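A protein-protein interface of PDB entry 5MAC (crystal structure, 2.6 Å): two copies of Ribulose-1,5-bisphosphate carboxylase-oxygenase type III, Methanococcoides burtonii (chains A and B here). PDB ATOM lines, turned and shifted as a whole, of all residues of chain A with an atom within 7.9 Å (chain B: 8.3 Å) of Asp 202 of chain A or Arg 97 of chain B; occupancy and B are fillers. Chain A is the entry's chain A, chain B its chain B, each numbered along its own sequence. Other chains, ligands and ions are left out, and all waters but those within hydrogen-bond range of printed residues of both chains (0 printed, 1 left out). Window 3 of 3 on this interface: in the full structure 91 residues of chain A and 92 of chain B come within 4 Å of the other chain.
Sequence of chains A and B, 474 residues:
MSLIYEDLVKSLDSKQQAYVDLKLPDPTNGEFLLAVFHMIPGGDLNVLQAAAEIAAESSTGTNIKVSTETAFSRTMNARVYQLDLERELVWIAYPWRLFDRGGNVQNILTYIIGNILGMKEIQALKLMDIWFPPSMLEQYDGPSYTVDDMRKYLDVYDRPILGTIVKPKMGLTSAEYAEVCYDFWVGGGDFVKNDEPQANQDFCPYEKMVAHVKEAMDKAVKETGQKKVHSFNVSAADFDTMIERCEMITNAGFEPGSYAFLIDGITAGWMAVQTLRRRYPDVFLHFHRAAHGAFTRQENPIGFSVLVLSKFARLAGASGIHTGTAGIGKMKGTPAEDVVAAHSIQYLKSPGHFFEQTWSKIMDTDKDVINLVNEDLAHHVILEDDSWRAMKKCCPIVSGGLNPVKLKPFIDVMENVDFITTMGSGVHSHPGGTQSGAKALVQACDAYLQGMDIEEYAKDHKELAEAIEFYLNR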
ATOM      1  N   MET A 170       5.968 -26.729  -0.008  1.00  0.00           N
ATOM      2  CA  MET A 170       5.623 -27.287  -1.311  1.00  0.00           C
ATOM      3  C   MET A 170       5.719 -28.801  -1.193  1.00  0.00           C
ATOM      4  O   MET A 170       6.453 -29.305  -0.346  1.00  0.00           O
ATOM      5  CB  MET A 170       6.597 -26.736  -2.397  1.00  0.00           C
ATOM      6  CG  MET A 170       6.236 -27.114  -3.820  1.00  0.00           C
ATOM      7  SD  MET A 170       4.503 -26.848  -4.297  1.00  0.00           S
ATOM      8  CE  MET A 170       4.322 -25.178  -3.923  1.00  0.00           C
ATOM      9  N   GLY A 171       4.960 -29.506  -2.021  1.00  0.00           N
ATOM     10  CA  GLY A 171       4.886 -30.965  -2.015  1.00  0.00           C
ATOM     11  C   GLY A 171       3.527 -31.538  -1.645  1.00  0.00           C
ATOM     12  O   GLY A 171       3.222 -32.668  -2.038  1.00  0.00           O
ATOM     13  N   THR A 173      -0.581 -31.954  -1.834  1.00  0.00           N
ATOM     14  CA  THR A 173      -1.618 -31.853  -2.850  1.00  0.00           C
ATOM     15  C   THR A 173      -2.694 -30.872  -2.395  1.00  0.00           C
ATOM     16  O   THR A 173      -2.671 -30.385  -1.261  1.00  0.00           O
ATOM     17  CB  THR A 173      -2.183 -33.239  -3.151  1.00  0.00           C
ATOM     18  OG1 THR A 173      -2.724 -33.787  -1.948  1.00  0.00           O
ATOM     19  CG2 THR A 173      -1.130 -34.164  -3.705  1.00  0.00           C
ATOM     20  N   SER A 174      -3.632 -30.589  -3.294  1.00  0.00           N
ATOM     21  CA  SER A 174      -4.751 -29.683  -3.043  1.00  0.00           C
ATOM     22  C   SER A 174      -5.673 -30.190  -1.933  1.00  0.00           C
ATOM     23  O   SER A 174      -6.266 -29.387  -1.221  1.00  0.00           O
ATOM     24  CB  SER A 174      -5.525 -29.431  -4.333  1.00  0.00           C
ATOM     25  OG  SER A 174      -5.350 -30.511  -5.232  1.00  0.00           O
ATOM     26  N   ALA A 199       1.036 -22.221  -5.405  1.00  0.00           N
ATOM     27  CA  ALA A 199       0.207 -21.746  -6.508  1.00  0.00           C
ATOM     28  C   ALA A 199      -0.362 -22.916  -7.350  1.00  0.00           C
ATOM     29  O   ALA A 199      -0.966 -23.841  -6.781  1.00  0.00           O
ATOM     30  CB  ALA A 199       1.043 -20.809  -7.356  1.00  0.00           C
ATOM     31  N   ASN A 200      -0.225 -22.867  -8.686  1.00  0.00           N
ATOM     32  CA  ASN A 200      -0.727 -23.913  -9.565  1.00  0.00           C
ATOM     33  C   ASN A 200       0.371 -24.885  -9.996  1.00  0.00           C
ATOM     34  O   ASN A 200       0.741 -24.921 -11.163  1.00  0.00           O
ATOM     35  CB  ASN A 200      -1.401 -23.264 -10.772  1.00  0.00           C
ATOM     36  CG  ASN A 200      -2.261 -24.198 -11.555  1.00  0.00           C
ATOM     37  OD1 ASN A 200      -2.961 -25.058 -10.999  1.00  0.00           O
ATOM     38  ND2 ASN A 200      -2.289 -23.984 -12.858  1.00  0.00           N
ATOM     39  N   GLN A 201       0.880 -25.685  -9.053  1.00  0.00           N
ATOM     40  CA  GLN A 201       1.874 -26.710  -9.356  1.00  0.00           C
ATOM     41  C   GLN A 201       1.082 -27.906  -9.851  1.00  0.00           C
ATOM     42  O   GLN A 201      -0.101 -28.028  -9.519  1.00  0.00           O
ATOM     43  CB  GLN A 201       2.774 -27.050  -8.151  1.00  0.00           C
ATOM     44  CG  GLN A 201       3.878 -26.005  -7.869  1.00  0.00           C
ATOM     45  CD  GLN A 201       3.421 -24.748  -7.174  1.00  0.00           C
ATOM     46  OE1 GLN A 201       2.284 -24.620  -6.715  1.00  0.00           O
ATOM     47  NE2 GLN A 201       4.340 -23.828  -6.980  1.00  0.00           N
ATOM     48  N   ASP A 202       1.711 -28.753 -10.690  1.00  0.00           N
ATOM     49  CA  ASP A 202       1.067 -29.891 -11.356  1.00  0.00           C
ATOM     50  C   ASP A 202       0.301 -30.859 -10.421  1.00  0.00           C
ATOM     51  O   ASP A 202      -0.736 -31.399 -10.811  1.00  0.00           O
ATOM     52  CB  ASP A 202       2.101 -30.667 -12.211  1.00  0.00           C
ATOM     53  CG  ASP A 202       3.166 -31.411 -11.425  1.00  0.00           C
ATOM     54  OD1 ASP A 202       4.294 -30.881 -11.303  1.00  0.00           O
ATOM     55  OD2 ASP A 202       2.884 -32.539 -10.967  1.00  0.00           O
ATOM     56  N   PHE A 203       0.783 -31.026  -9.192  1.00  0.00           N
ATOM     57  CA  PHE A 203       0.202 -31.942  -8.196  1.00  0.00           C
ATOM     58  C   PHE A 203      -0.782 -31.275  -7.202  1.00  0.00           C
ATOM     59  O   PHE A 203      -1.278 -31.947  -6.300  1.00  0.00           O
ATOM     60  CB  PHE A 203       1.313 -32.682  -7.437  1.00  0.00           C
ATOM     61  CG  PHE A 203       2.349 -31.758  -6.868  1.00  0.00           C
ATOM     62  CD1 PHE A 203       2.169 -31.170  -5.628  1.00  0.00           C
ATOM     63  CD2 PHE A 203       3.468 -31.414  -7.605  1.00  0.00           C
ATOM     64  CE1 PHE A 203       3.087 -30.251  -5.140  1.00  0.00           C
ATOM     65  CE2 PHE A 203       4.364 -30.481  -7.137  1.00  0.00           C
ATOM     66  CZ  PHE A 203       4.186 -29.915  -5.900  1.00  0.00           C
ATOM     67  N   CYS A 204      -1.064 -29.973  -7.380  1.00  0.00           N
ATOM     68  CA  CYS A 204      -1.960 -29.193  -6.531  1.00  0.00           C
ATOM     69  C   CYS A 204      -2.745 -28.224  -7.437  1.00  0.00           C
ATOM     70  O   CYS A 204      -2.480 -27.026  -7.413  1.00  0.00           O
ATOM     71  CB  CYS A 204      -1.148 -28.452  -5.466  1.00  0.00           C
ATOM     72  SG  CYS A 204      -2.150 -27.644  -4.188  1.00  0.00           S
ATOM     73  N   PRO A 205      -3.669 -28.738  -8.293  1.00  0.00           N
ATOM     74  CA  PRO A 205      -4.411 -27.839  -9.184  1.00  0.00           C
ATOM     75  C   PRO A 205      -5.099 -26.772  -8.378  1.00  0.00           C
ATOM     76  O   PRO A 205      -5.771 -27.088  -7.397  1.00  0.00           O
ATOM     77  CB  PRO A 205      -5.402 -28.777  -9.890  1.00  0.00           C
ATOM     78  CG  PRO A 205      -4.766 -30.110  -9.827  1.00  0.00           C
ATOM     79  CD  PRO A 205      -4.114 -30.140  -8.481  1.00  0.00           C
ATOM     80  N   TYR A 206      -4.848 -25.512  -8.735  1.00  0.00           N
ATOM     81  CA  TYR A 206      -5.367 -24.343  -8.006  1.00  0.00           C
ATOM     82  C   TYR A 206      -6.868 -24.425  -7.783  1.00  0.00           C
ATOM     83  O   TYR A 206      -7.334 -24.133  -6.697  1.00  0.00           O
ATOM     84  CB  TYR A 206      -5.028 -23.043  -8.781  1.00  0.00           C
ATOM     85  CG  TYR A 206      -5.011 -21.792  -7.932  1.00  0.00           C
ATOM     86  CD1 TYR A 206      -3.868 -21.417  -7.238  1.00  0.00           C
ATOM     87  CD2 TYR A 206      -6.121 -20.960  -7.859  1.00  0.00           C
ATOM     88  CE1 TYR A 206      -3.838 -20.256  -6.469  1.00  0.00           C
ATOM     89  CE2 TYR A 206      -6.095 -19.786  -7.112  1.00  0.00           C
ATOM     90  CZ  TYR A 206      -4.945 -19.429  -6.437  1.00  0.00           C
ATOM     91  OH  TYR A 206      -4.934 -18.294  -5.689  1.00  0.00           O
ATOM     92  N   GLY B  30      18.005 -32.989 -15.754  1.00  0.00           N
ATOM     93  CA  GLY B  30      16.791 -32.312 -16.200  1.00  0.00           C
ATOM     94  C   GLY B  30      15.766 -32.098 -15.115  1.00  0.00           C
ATOM     95  O   GLY B  30      14.924 -31.217 -15.242  1.00  0.00           O
ATOM     96  N   GLU B  31      15.816 -32.901 -14.046  1.00  0.00           N
ATOM     97  CA  GLU B  31      14.889 -32.770 -12.918  1.00  0.00           C
ATOM     98  C   GLU B  31      15.044 -31.463 -12.203  1.00  0.00           C
ATOM     99  O   GLU B  31      14.066 -31.018 -11.614  1.00  0.00           O
ATOM    100  CB  GLU B  31      15.107 -33.863 -11.864  1.00  0.00           C
ATOM    101  CG  GLU B  31      14.785 -35.261 -12.316  1.00  0.00           C
ATOM    102  CD  GLU B  31      14.745 -36.236 -11.158  1.00  0.00           C
ATOM    103  OE1 GLU B  31      15.826 -36.661 -10.686  1.00  0.00           O
ATOM    104  OE2 GLU B  31      13.623 -36.562 -10.712  1.00  0.00           O
ATOM    105  N   PHE B  32      16.273 -30.874 -12.209  1.00  0.00           N
ATOM    106  CA  PHE B  32      16.628 -29.698 -11.444  1.00  0.00           C
ATOM    107  C   PHE B  32      17.114 -28.443 -12.180  1.00  0.00           C
ATOM    108  O   PHE B  32      17.830 -28.519 -13.161  1.00  0.00           O
ATOM    109  CB  PHE B  32      17.778 -30.087 -10.490  1.00  0.00           C
ATOM    110  CG  PHE B  32      17.695 -31.452  -9.867  1.00  0.00           C
ATOM    111  CD1 PHE B  32      16.971 -31.656  -8.709  1.00  0.00           C
ATOM    112  CD2 PHE B  32      18.402 -32.516 -10.395  1.00  0.00           C
ATOM    113  CE1 PHE B  32      16.906 -32.912  -8.119  1.00  0.00           C
ATOM    114  CE2 PHE B  32      18.337 -33.773  -9.807  1.00  0.00           C
ATOM    115  CZ  PHE B  32      17.579 -33.964  -8.673  1.00  0.00           C
ATOM    116  N   LEU B  33      16.886 -27.303 -11.525  1.00  0.00           N
ATOM    117  CA  LEU B  33      17.410 -25.971 -11.799  1.00  0.00           C
ATOM    118  C   LEU B  33      18.598 -25.982 -10.852  1.00  0.00           C
ATOM    119  O   LEU B  33      18.456 -26.386  -9.680  1.00  0.00           O
ATOM    120  CB  LEU B  33      16.356 -24.905 -11.368  1.00  0.00           C
ATOM    121  CG  LEU B  33      16.667 -23.382 -11.348  1.00  0.00           C
ATOM    122  CD1 LEU B  33      17.380 -22.949 -10.075  1.00  0.00           C
ATOM    123  CD2 LEU B  33      17.399 -22.946 -12.540  1.00  0.00           C
ATOM    124  N   PHE B  72       5.940 -37.917  -0.560  1.00  0.00           N
ATOM    125  CA  PHE B  72       5.906 -37.277  -1.872  1.00  0.00           C
ATOM    126  C   PHE B  72       6.491 -35.875  -1.808  1.00  0.00           C
ATOM    127  O   PHE B  72       7.105 -35.429  -2.776  1.00  0.00           O
ATOM    128  CB  PHE B  72       4.470 -37.259  -2.448  1.00  0.00           C
ATOM    129  CG  PHE B  72       4.347 -36.678  -3.836  1.00  0.00           C
ATOM    130  CD1 PHE B  72       4.667 -37.433  -4.957  1.00  0.00           C
ATOM    131  CD2 PHE B  72       3.975 -35.356  -4.021  1.00  0.00           C
ATOM    132  CE1 PHE B  72       4.615 -36.874  -6.235  1.00  0.00           C
ATOM    133  CE2 PHE B  72       3.903 -34.802  -5.300  1.00  0.00           C
ATOM    134  CZ  PHE B  72       4.220 -35.562  -6.401  1.00  0.00           C
ATOM    135  N   THR B  75      10.317 -35.661  -2.208  1.00  0.00           N
ATOM    136  CA  THR B  75      10.829 -35.790  -3.584  1.00  0.00           C
ATOM    137  C   THR B  75      11.035 -34.413  -4.260  1.00  0.00           C
ATOM    138  O   THR B  75      11.684 -34.320  -5.307  1.00  0.00           O
ATOM    139  CB  THR B  75       9.898 -36.673  -4.451  1.00  0.00           C
ATOM    140  OG1 THR B  75       8.774 -35.927  -4.901  1.00  0.00           O
ATOM    141  CG2 THR B  75       9.426 -37.923  -3.741  1.00  0.00           C
ATOM    142  N   MET B  76      10.455 -33.368  -3.677  1.00  0.00           N
ATOM    143  CA  MET B  76      10.505 -32.006  -4.182  1.00  0.00           C
ATOM    144  C   MET B  76      11.574 -31.201  -3.436  1.00  0.00           C
ATOM    145  O   MET B  76      11.815 -30.046  -3.773  1.00  0.00           O
ATOM    146  CB  MET B  76       9.134 -31.351  -3.956  1.00  0.00           C
ATOM    147  CG  MET B  76       7.950 -32.153  -4.478  1.00  0.00           C
ATOM    148  SD  MET B  76       7.922 -32.210  -6.266  1.00  0.00           S
ATOM    149  CE  MET B  76       7.827 -30.492  -6.578  1.00  0.00           C
ATOM    150  N   TYR B  94      17.587 -27.580  -7.369  1.00  0.00           N
ATOM    151  CA  TYR B  94      16.169 -27.283  -7.146  1.00  0.00           C
ATOM    152  C   TYR B  94      15.213 -28.043  -8.101  1.00  0.00           C
ATOM    153  O   TYR B  94      15.067 -27.634  -9.258  1.00  0.00           O
ATOM    154  CB  TYR B  94      15.924 -25.758  -7.299  1.00  0.00           C
ATOM    155  CG  TYR B  94      16.468 -24.917  -6.170  1.00  0.00           C
ATOM    156  CD1 TYR B  94      17.725 -24.334  -6.253  1.00  0.00           C
ATOM    157  CD2 TYR B  94      15.702 -24.650  -5.048  1.00  0.00           C
ATOM    158  CE1 TYR B  94      18.230 -23.557  -5.212  1.00  0.00           C
ATOM    159  CE2 TYR B  94      16.209 -23.907  -3.989  1.00  0.00           C
ATOM    160  CZ  TYR B  94      17.477 -23.358  -4.074  1.00  0.00           C
ATOM    161  OH  TYR B  94      17.981 -22.575  -3.061  1.00  0.00           O
ATOM    162  N   PRO B  95      14.440 -29.041  -7.604  1.00  0.00           N
ATOM    163  CA  PRO B  95      13.455 -29.708  -8.470  1.00  0.00           C
ATOM    164  C   PRO B  95      12.522 -28.699  -9.122  1.00  0.00           C
ATOM    165  O   PRO B  95      11.750 -28.077  -8.402  1.00  0.00           O
ATOM    166  CB  PRO B  95      12.713 -30.631  -7.483  1.00  0.00           C
ATOM    167  CG  PRO B  95      13.748 -30.948  -6.461  1.00  0.00           C
ATOM    168  CD  PRO B  95      14.453 -29.646  -6.254  1.00  0.00           C
ATOM    169  N   TRP B  96      12.569 -28.519 -10.461  1.00  0.00           N
ATOM    170  CA  TRP B  96      11.726 -27.484 -11.091  1.00  0.00           C
ATOM    171  C   TRP B  96      10.205 -27.787 -11.051  1.00  0.00           C
ATOM    172  O   TRP B  96       9.425 -26.928 -11.435  1.00  0.00           O
ATOM    173  CB  TRP B  96      12.195 -27.091 -12.515  1.00  0.00           C
ATOM    174  CG  TRP B  96      12.180 -28.138 -13.578  1.00  0.00           C
ATOM    175  CD1 TRP B  96      13.261 -28.795 -14.075  1.00  0.00           C
ATOM    176  CD2 TRP B  96      11.087 -28.444 -14.458  1.00  0.00           C
ATOM    177  NE1 TRP B  96      12.909 -29.505 -15.196  1.00  0.00           N
ATOM    178  CE2 TRP B  96      11.564 -29.373 -15.403  1.00  0.00           C
ATOM    179  CE3 TRP B  96       9.718 -28.120 -14.466  1.00  0.00           C
ATOM    180  CZ2 TRP B  96      10.741 -29.943 -16.371  1.00  0.00           C
ATOM    181  CZ3 TRP B  96       8.896 -28.711 -15.416  1.00  0.00           C
ATOM    182  CH2 TRP B  96       9.411 -29.613 -16.348  1.00  0.00           C
ATOM    183  N   ARG B  97       9.784 -28.949 -10.531  1.00  0.00           N
ATOM    184  CA  ARG B  97       8.382 -29.239 -10.260  1.00  0.00           C
ATOM    185  C   ARG B  97       7.870 -28.355  -9.073  1.00  0.00           C
ATOM    186  O   ARG B  97       6.668 -28.226  -8.887  1.00  0.00           O
ATOM    187  CB  ARG B  97       8.152 -30.725  -9.959  1.00  0.00           C
ATOM    188  CG  ARG B  97       8.001 -31.582 -11.187  1.00  0.00           C
ATOM    189  CD  ARG B  97       7.680 -33.014 -10.790  1.00  0.00           C
ATOM    190  NE  ARG B  97       6.256 -33.262 -10.579  1.00  0.00           N
ATOM    191  CZ  ARG B  97       5.755 -34.450 -10.253  1.00  0.00           C
ATOM    192  NH1 ARG B  97       6.554 -35.500 -10.102  1.00  0.00           N
ATOM    193  NH2 ARG B  97       4.449 -34.598 -10.076  1.00  0.00           N
ATOM    194  N   LEU B  98       8.780 -27.794  -8.246  1.00  0.00           N
ATOM    195  CA  LEU B  98       8.443 -26.840  -7.176  1.00  0.00           C
ATOM    196  C   LEU B  98       7.778 -25.582  -7.751  1.00  0.00           C
ATOM    197  O   LEU B  98       6.936 -24.964  -7.091  1.00  0.00           O
ATOM    198  CB  LEU B  98       9.729 -26.348  -6.477  1.00  0.00           C
ATOM    199  CG  LEU B  98      10.455 -27.275  -5.525  1.00  0.00           C
ATOM    200  CD1 LEU B  98      11.742 -26.655  -5.107  1.00  0.00           C
ATOM    201  CD2 LEU B  98       9.627 -27.536  -4.280  1.00  0.00           C
ATOM    202  N   PHE B  99       8.200 -25.170  -8.951  1.00  0.00           N
ATOM    203  CA  PHE B  99       7.738 -23.928  -9.567  1.00  0.00           C
ATOM    204  C   PHE B  99       6.295 -23.964 -10.128  1.00  0.00           C
ATOM    205  O   PHE B  99       5.849 -24.950 -10.718  1.00  0.00           O
ATOM    206  CB  PHE B  99       8.730 -23.445 -10.657  1.00  0.00           C
ATOM    207  CG  PHE B  99      10.194 -23.495 -10.282  1.00  0.00           C
ATOM    208  CD1 PHE B  99      10.606 -23.278  -8.968  1.00  0.00           C
ATOM    209  CD2 PHE B  99      11.159 -23.789 -11.232  1.00  0.00           C
ATOM    210  CE1 PHE B  99      11.943 -23.394  -8.611  1.00  0.00           C
ATOM    211  CE2 PHE B  99      12.506 -23.851 -10.880  1.00  0.00           C
ATOM    212  CZ  PHE B  99      12.882 -23.696  -9.565  1.00  0.00           C
ATOM    213  N   ASP B 100       5.589 -22.835  -9.948  1.00  0.00           N
ATOM    214  CA  ASP B 100       4.229 -22.599 -10.435  1.00  0.00           C
ATOM    215  C   ASP B 100       4.241 -22.687 -11.956  1.00  0.00           C
ATOM    216  O   ASP B 100       5.163 -22.185 -12.623  1.00  0.00           O
ATOM    217  CB  ASP B 100       3.710 -21.215  -9.986  1.00  0.00           C
ATOM    218  CG  ASP B 100       2.340 -20.800 -10.504  1.00  0.00           C
ATOM    219  OD1 ASP B 100       2.107 -19.578 -10.662  1.00  0.00           O
ATOM    220  OD2 ASP B 100       1.500 -21.690 -10.756  1.00  0.00           O
ATOM    221  N   ARG B 101       3.170 -23.292 -12.475  1.00  0.00           N
ATOM    222  CA  ARG B 101       2.996 -23.589 -13.877  1.00  0.00           C
ATOM    223  C   ARG B 101       2.527 -22.403 -14.674  1.00  0.00           C
ATOM    224  O   ARG B 101       2.300 -21.313 -14.141  1.00  0.00           O
ATOM    225  CB  ARG B 101       2.085 -24.809 -14.036  1.00  0.00           C
ATOM    226  CG  ARG B 101       2.689 -26.067 -13.396  1.00  0.00           C
ATOM    227  CD  ARG B 101       3.721 -26.682 -14.315  1.00  0.00           C
ATOM    228  NE  ARG B 101       4.372 -27.838 -13.709  1.00  0.00           N
ATOM    229  CZ  ARG B 101       5.019 -28.783 -14.384  1.00  0.00           C
ATOM    230  NH1 ARG B 101       5.121 -28.715 -15.708  1.00  0.00           N
ATOM    231  NH2 ARG B 101       5.565 -29.809 -13.741  1.00  0.00           N
ATOM    232  N   GLY B 102       2.543 -22.593 -15.982  1.00  0.00           N
ATOM    233  CA  GLY B 102       2.300 -21.531 -16.942  1.00  0.00           C
ATOM    234  C   GLY B 102       3.495 -20.608 -17.104  1.00  0.00           C
ATOM    235  O   GLY B 102       3.315 -19.474 -17.538  1.00  0.00           O
ATOM    236  N   ASN B 107       7.755 -16.651  -9.234  1.00  0.00           N
ATOM    237  CA  ASN B 107       7.665 -17.804  -8.349  1.00  0.00           C
ATOM    238  C   ASN B 107       9.033 -18.454  -8.156  1.00  0.00           C
ATOM    239  O   ASN B 107       9.364 -18.827  -7.032  1.00  0.00           O
ATOM    240  CB  ASN B 107       6.643 -18.794  -8.914  1.00  0.00           C
ATOM    241  CG  ASN B 107       6.285 -19.882  -7.967  1.00  0.00           C
ATOM    242  OD1 ASN B 107       6.613 -21.033  -8.209  1.00  0.00           O
ATOM    243  ND2 ASN B 107       5.515 -19.578  -6.923  1.00  0.00           N
ATOM    244  N   TYR B 111      11.400 -18.423  -4.400  1.00  0.00           N
ATOM    245  CA  TYR B 111      12.118 -19.485  -3.745  1.00  0.00           C
ATOM    246  C   TYR B 111      13.618 -19.154  -3.521  1.00  0.00           C
ATOM    247  O   TYR B 111      14.114 -19.149  -2.380  1.00  0.00           O
ATOM    248  CB  TYR B 111      12.059 -20.774  -4.575  1.00  0.00           C
ATOM    249  CG  TYR B 111      10.757 -21.548  -4.543  1.00  0.00           C
ATOM    250  CD1 TYR B 111      10.425 -22.346  -3.450  1.00  0.00           C
ATOM    251  CD2 TYR B 111       9.949 -21.638  -5.679  1.00  0.00           C
ATOM    252  CE1 TYR B 111       9.254 -23.101  -3.437  1.00  0.00           C
ATOM    253  CE2 TYR B 111       8.811 -22.435  -5.693  1.00  0.00           C
ATOM    254  CZ  TYR B 111       8.495 -23.200  -4.580  1.00  0.00           C
ATOM    255  OH  TYR B 111       7.389 -23.988  -4.540  1.00  0.00           O
ATOM    256  N   MET B 136      13.205 -27.760 -18.429  1.00  0.00           N
ATOM    257  CA  MET B 136      12.673 -26.588 -17.748  1.00  0.00           C
ATOM    258  C   MET B 136      12.581 -25.428 -18.717  1.00  0.00           C
ATOM    259  O   MET B 136      11.540 -24.815 -18.828  1.00  0.00           O
ATOM    260  CB  MET B 136      13.589 -26.199 -16.590  1.00  0.00           C
ATOM    261  CG  MET B 136      13.012 -25.123 -15.705  1.00  0.00           C
ATOM    262  SD  MET B 136      14.265 -24.378 -14.670  1.00  0.00           S
ATOM    263  CE  MET B 136      13.540 -22.749 -14.412  1.00  0.00           C
ATOM    264  N   GLN B 139       9.368 -24.942 -20.567  1.00  0.00           N
ATOM    265  CA  GLN B 139       8.147 -24.523 -19.869  1.00  0.00           C
ATOM    266  C   GLN B 139       7.940 -23.002 -19.846  1.00  0.00           C
ATOM    267  O   GLN B 139       6.845 -22.557 -19.496  1.00  0.00           O
ATOM    268  CB  GLN B 139       8.179 -25.030 -18.422  1.00  0.00           C
ATOM    269  CG  GLN B 139       8.125 -26.547 -18.285  1.00  0.00           C
ATOM    270  CD  GLN B 139       6.712 -27.061 -18.468  1.00  0.00           C
ATOM    271  OE1 GLN B 139       5.820 -26.841 -17.622  1.00  0.00           O
ATOM    272  NE2 GLN B 139       6.458 -27.706 -19.599  1.00  0.00           N
ATOM    273  N   TYR B 140       8.983 -22.211 -20.196  1.00  0.00           N
ATOM    274  CA  TYR B 140       8.983 -20.762 -20.177  1.00  0.00           C
ATOM    275  C   TYR B 140       8.879 -20.203 -21.560  1.00  0.00           C
ATOM    276  O   TYR B 140       8.942 -20.936 -22.548  1.00  0.00           O
ATOM    277  CB  TYR B 140      10.221 -20.262 -19.423  1.00  0.00           C
ATOM    278  CG  TYR B 140      10.140 -20.670 -17.968  1.00  0.00           C
ATOM    279  CD1 TYR B 140       9.556 -19.830 -17.027  1.00  0.00           C
ATOM    280  CD2 TYR B 140      10.407 -21.980 -17.581  1.00  0.00           C
ATOM    281  CE1 TYR B 140       9.314 -20.258 -15.727  1.00  0.00           C
ATOM    282  CE2 TYR B 140      10.168 -22.419 -16.287  1.00  0.00           C
ATOM    283  CZ  TYR B 140       9.620 -21.557 -15.358  1.00  0.00           C
ATOM    284  OH  TYR B 140       9.406 -21.965 -14.056  1.00  0.00           O
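Among the printed residues, pairs that only touch across the chains: Met 170 of chain A with Tyr 111 of chain B, Ala 199 of chain A with Asp 100 of chain B, Gly 171 of chain A with Phe 72 of chain B, Met 170 of chain A with Leu 98 of chain B, Phe 203 of chain A with Met 76 of chain B, Gln 201 of chain A with Phe 99 of chain B, Phe 203 of chain A with Arg 97 of chain B, Gln 201 of chain A with Arg 97 of chain B, Phe 203 of chain A with Phe 72 of chain B, Gln 201 of chain A with Asn 107 of chain B and Gln 201 of chain A with Tyr 111 of chain B.
Asp 202 of chain A touches just these residues of chain B: Arg 97 and Arg 101. Arg 97 of chain B touches just these residues of chain A: Gln 201, Asp 202 and Phe 203. Of the printed residues of chain A, Phe 72 of chain B touches Gly 171 (3.4 Å) and Phe 203 (3.8 Å). Printed residues of chain A within 4 Å of Asp 100 of chain B: Ala 199, Asn 200 and Gln 201. Of the printed residues of chain B, Met 170 of chain A touches Leu 98 and Tyr 111.
O of Phe 72 of chain B lies within hydrogen-bond range of OG1 of Thr 75 of chain B. The side-chain hydroxyl (OH) of Tyr 111 of chain B sits at hydrogen-bond distance from the backbone carbonyl oxygen (O) of Leu 98 of chain B, at 2.8 Å. The backbone NH (N) of Ala 199 of chain A sits at hydrogen-bond distance from the side-chain amide oxygen (OE1) of Gln 201 of chain A (3.0 Å). OD1 of Asn 107 of chain B sits at hydrogen-bond distance from N of Asp 100 of chain B (2.7 Å). The guanidinium group of Arg 101 of chain B sits at hydrogen-bond distance from the side-chain amide oxygen of Gln 139 of chain B (2.8 Å). OD1 of Asn 200 of chain A lies within hydrogen-bond range of N of Tyr 206 of chain A.
The side-chain carboxylate (OD2) of Asp 202 of chain A lies within salt-bridge range of the guanidinium group (NH2) of Arg 97 of chain B. O of Asn 200 of chain A sits close to N of Arg 101 of chain B, at 3.2 Å. The backbone carbonyl oxygen (O) of Leu 98 of chain B lies within hydrogen-bond range of the side-chain amide nitrogen (NE2) of Gln 201 of chain A. OD1 of Asp 202 of chain A lies within salt-bridge range of NH2 of Arg 101 of chain B (3.0 Å). NE2 of Gln 201 of chain A sits close to N of Asp 100 of chain B (3.4 Å). The side-chain carboxylate of Asp 100 of chain B is in hydrogen-bond range of the backbone NH of Asn 200 of chain A (2.9 Å).
Of the 12 printed residues of chain A, 7 touch a printed residue of chain B. Hydrophobic or aromatic side chains of chain A within 4 Å of the printed part of chain B: Met 170, Ala 199 and Phe 203. Of the 21 printed residues of chain B, 9 touch a printed residue of chain A. Printed residues of chain B that touch a printed residue of chain A: Phe 72, Met 76, Arg 97, Leu 98, Phe 99, Asp 100, Arg 101, Asn 107 and Tyr 111. Hydrophobic or aromatic side chains of chain B within 4 Å of the printed part of chain A: Phe 72, Met 76, Leu 98 and Tyr 111. Along chain B the printed residues that touch a printed residue of chain A span positions 72 to 111. Among the printed residues, Asp or Glu carboxylates within 4 Å of a Lys or Arg side-chain nitrogen of the other chain: Asp 202 of chain A with Arg 97 of chain B (2.7 Å) and Asp 202 of chain A with Arg 101 of chain B (3.0 Å).
No position is printed for both chains. Of the 17 pairs that touch across the chains among the printed residues, none has its exchanged pair printed and touching as well.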
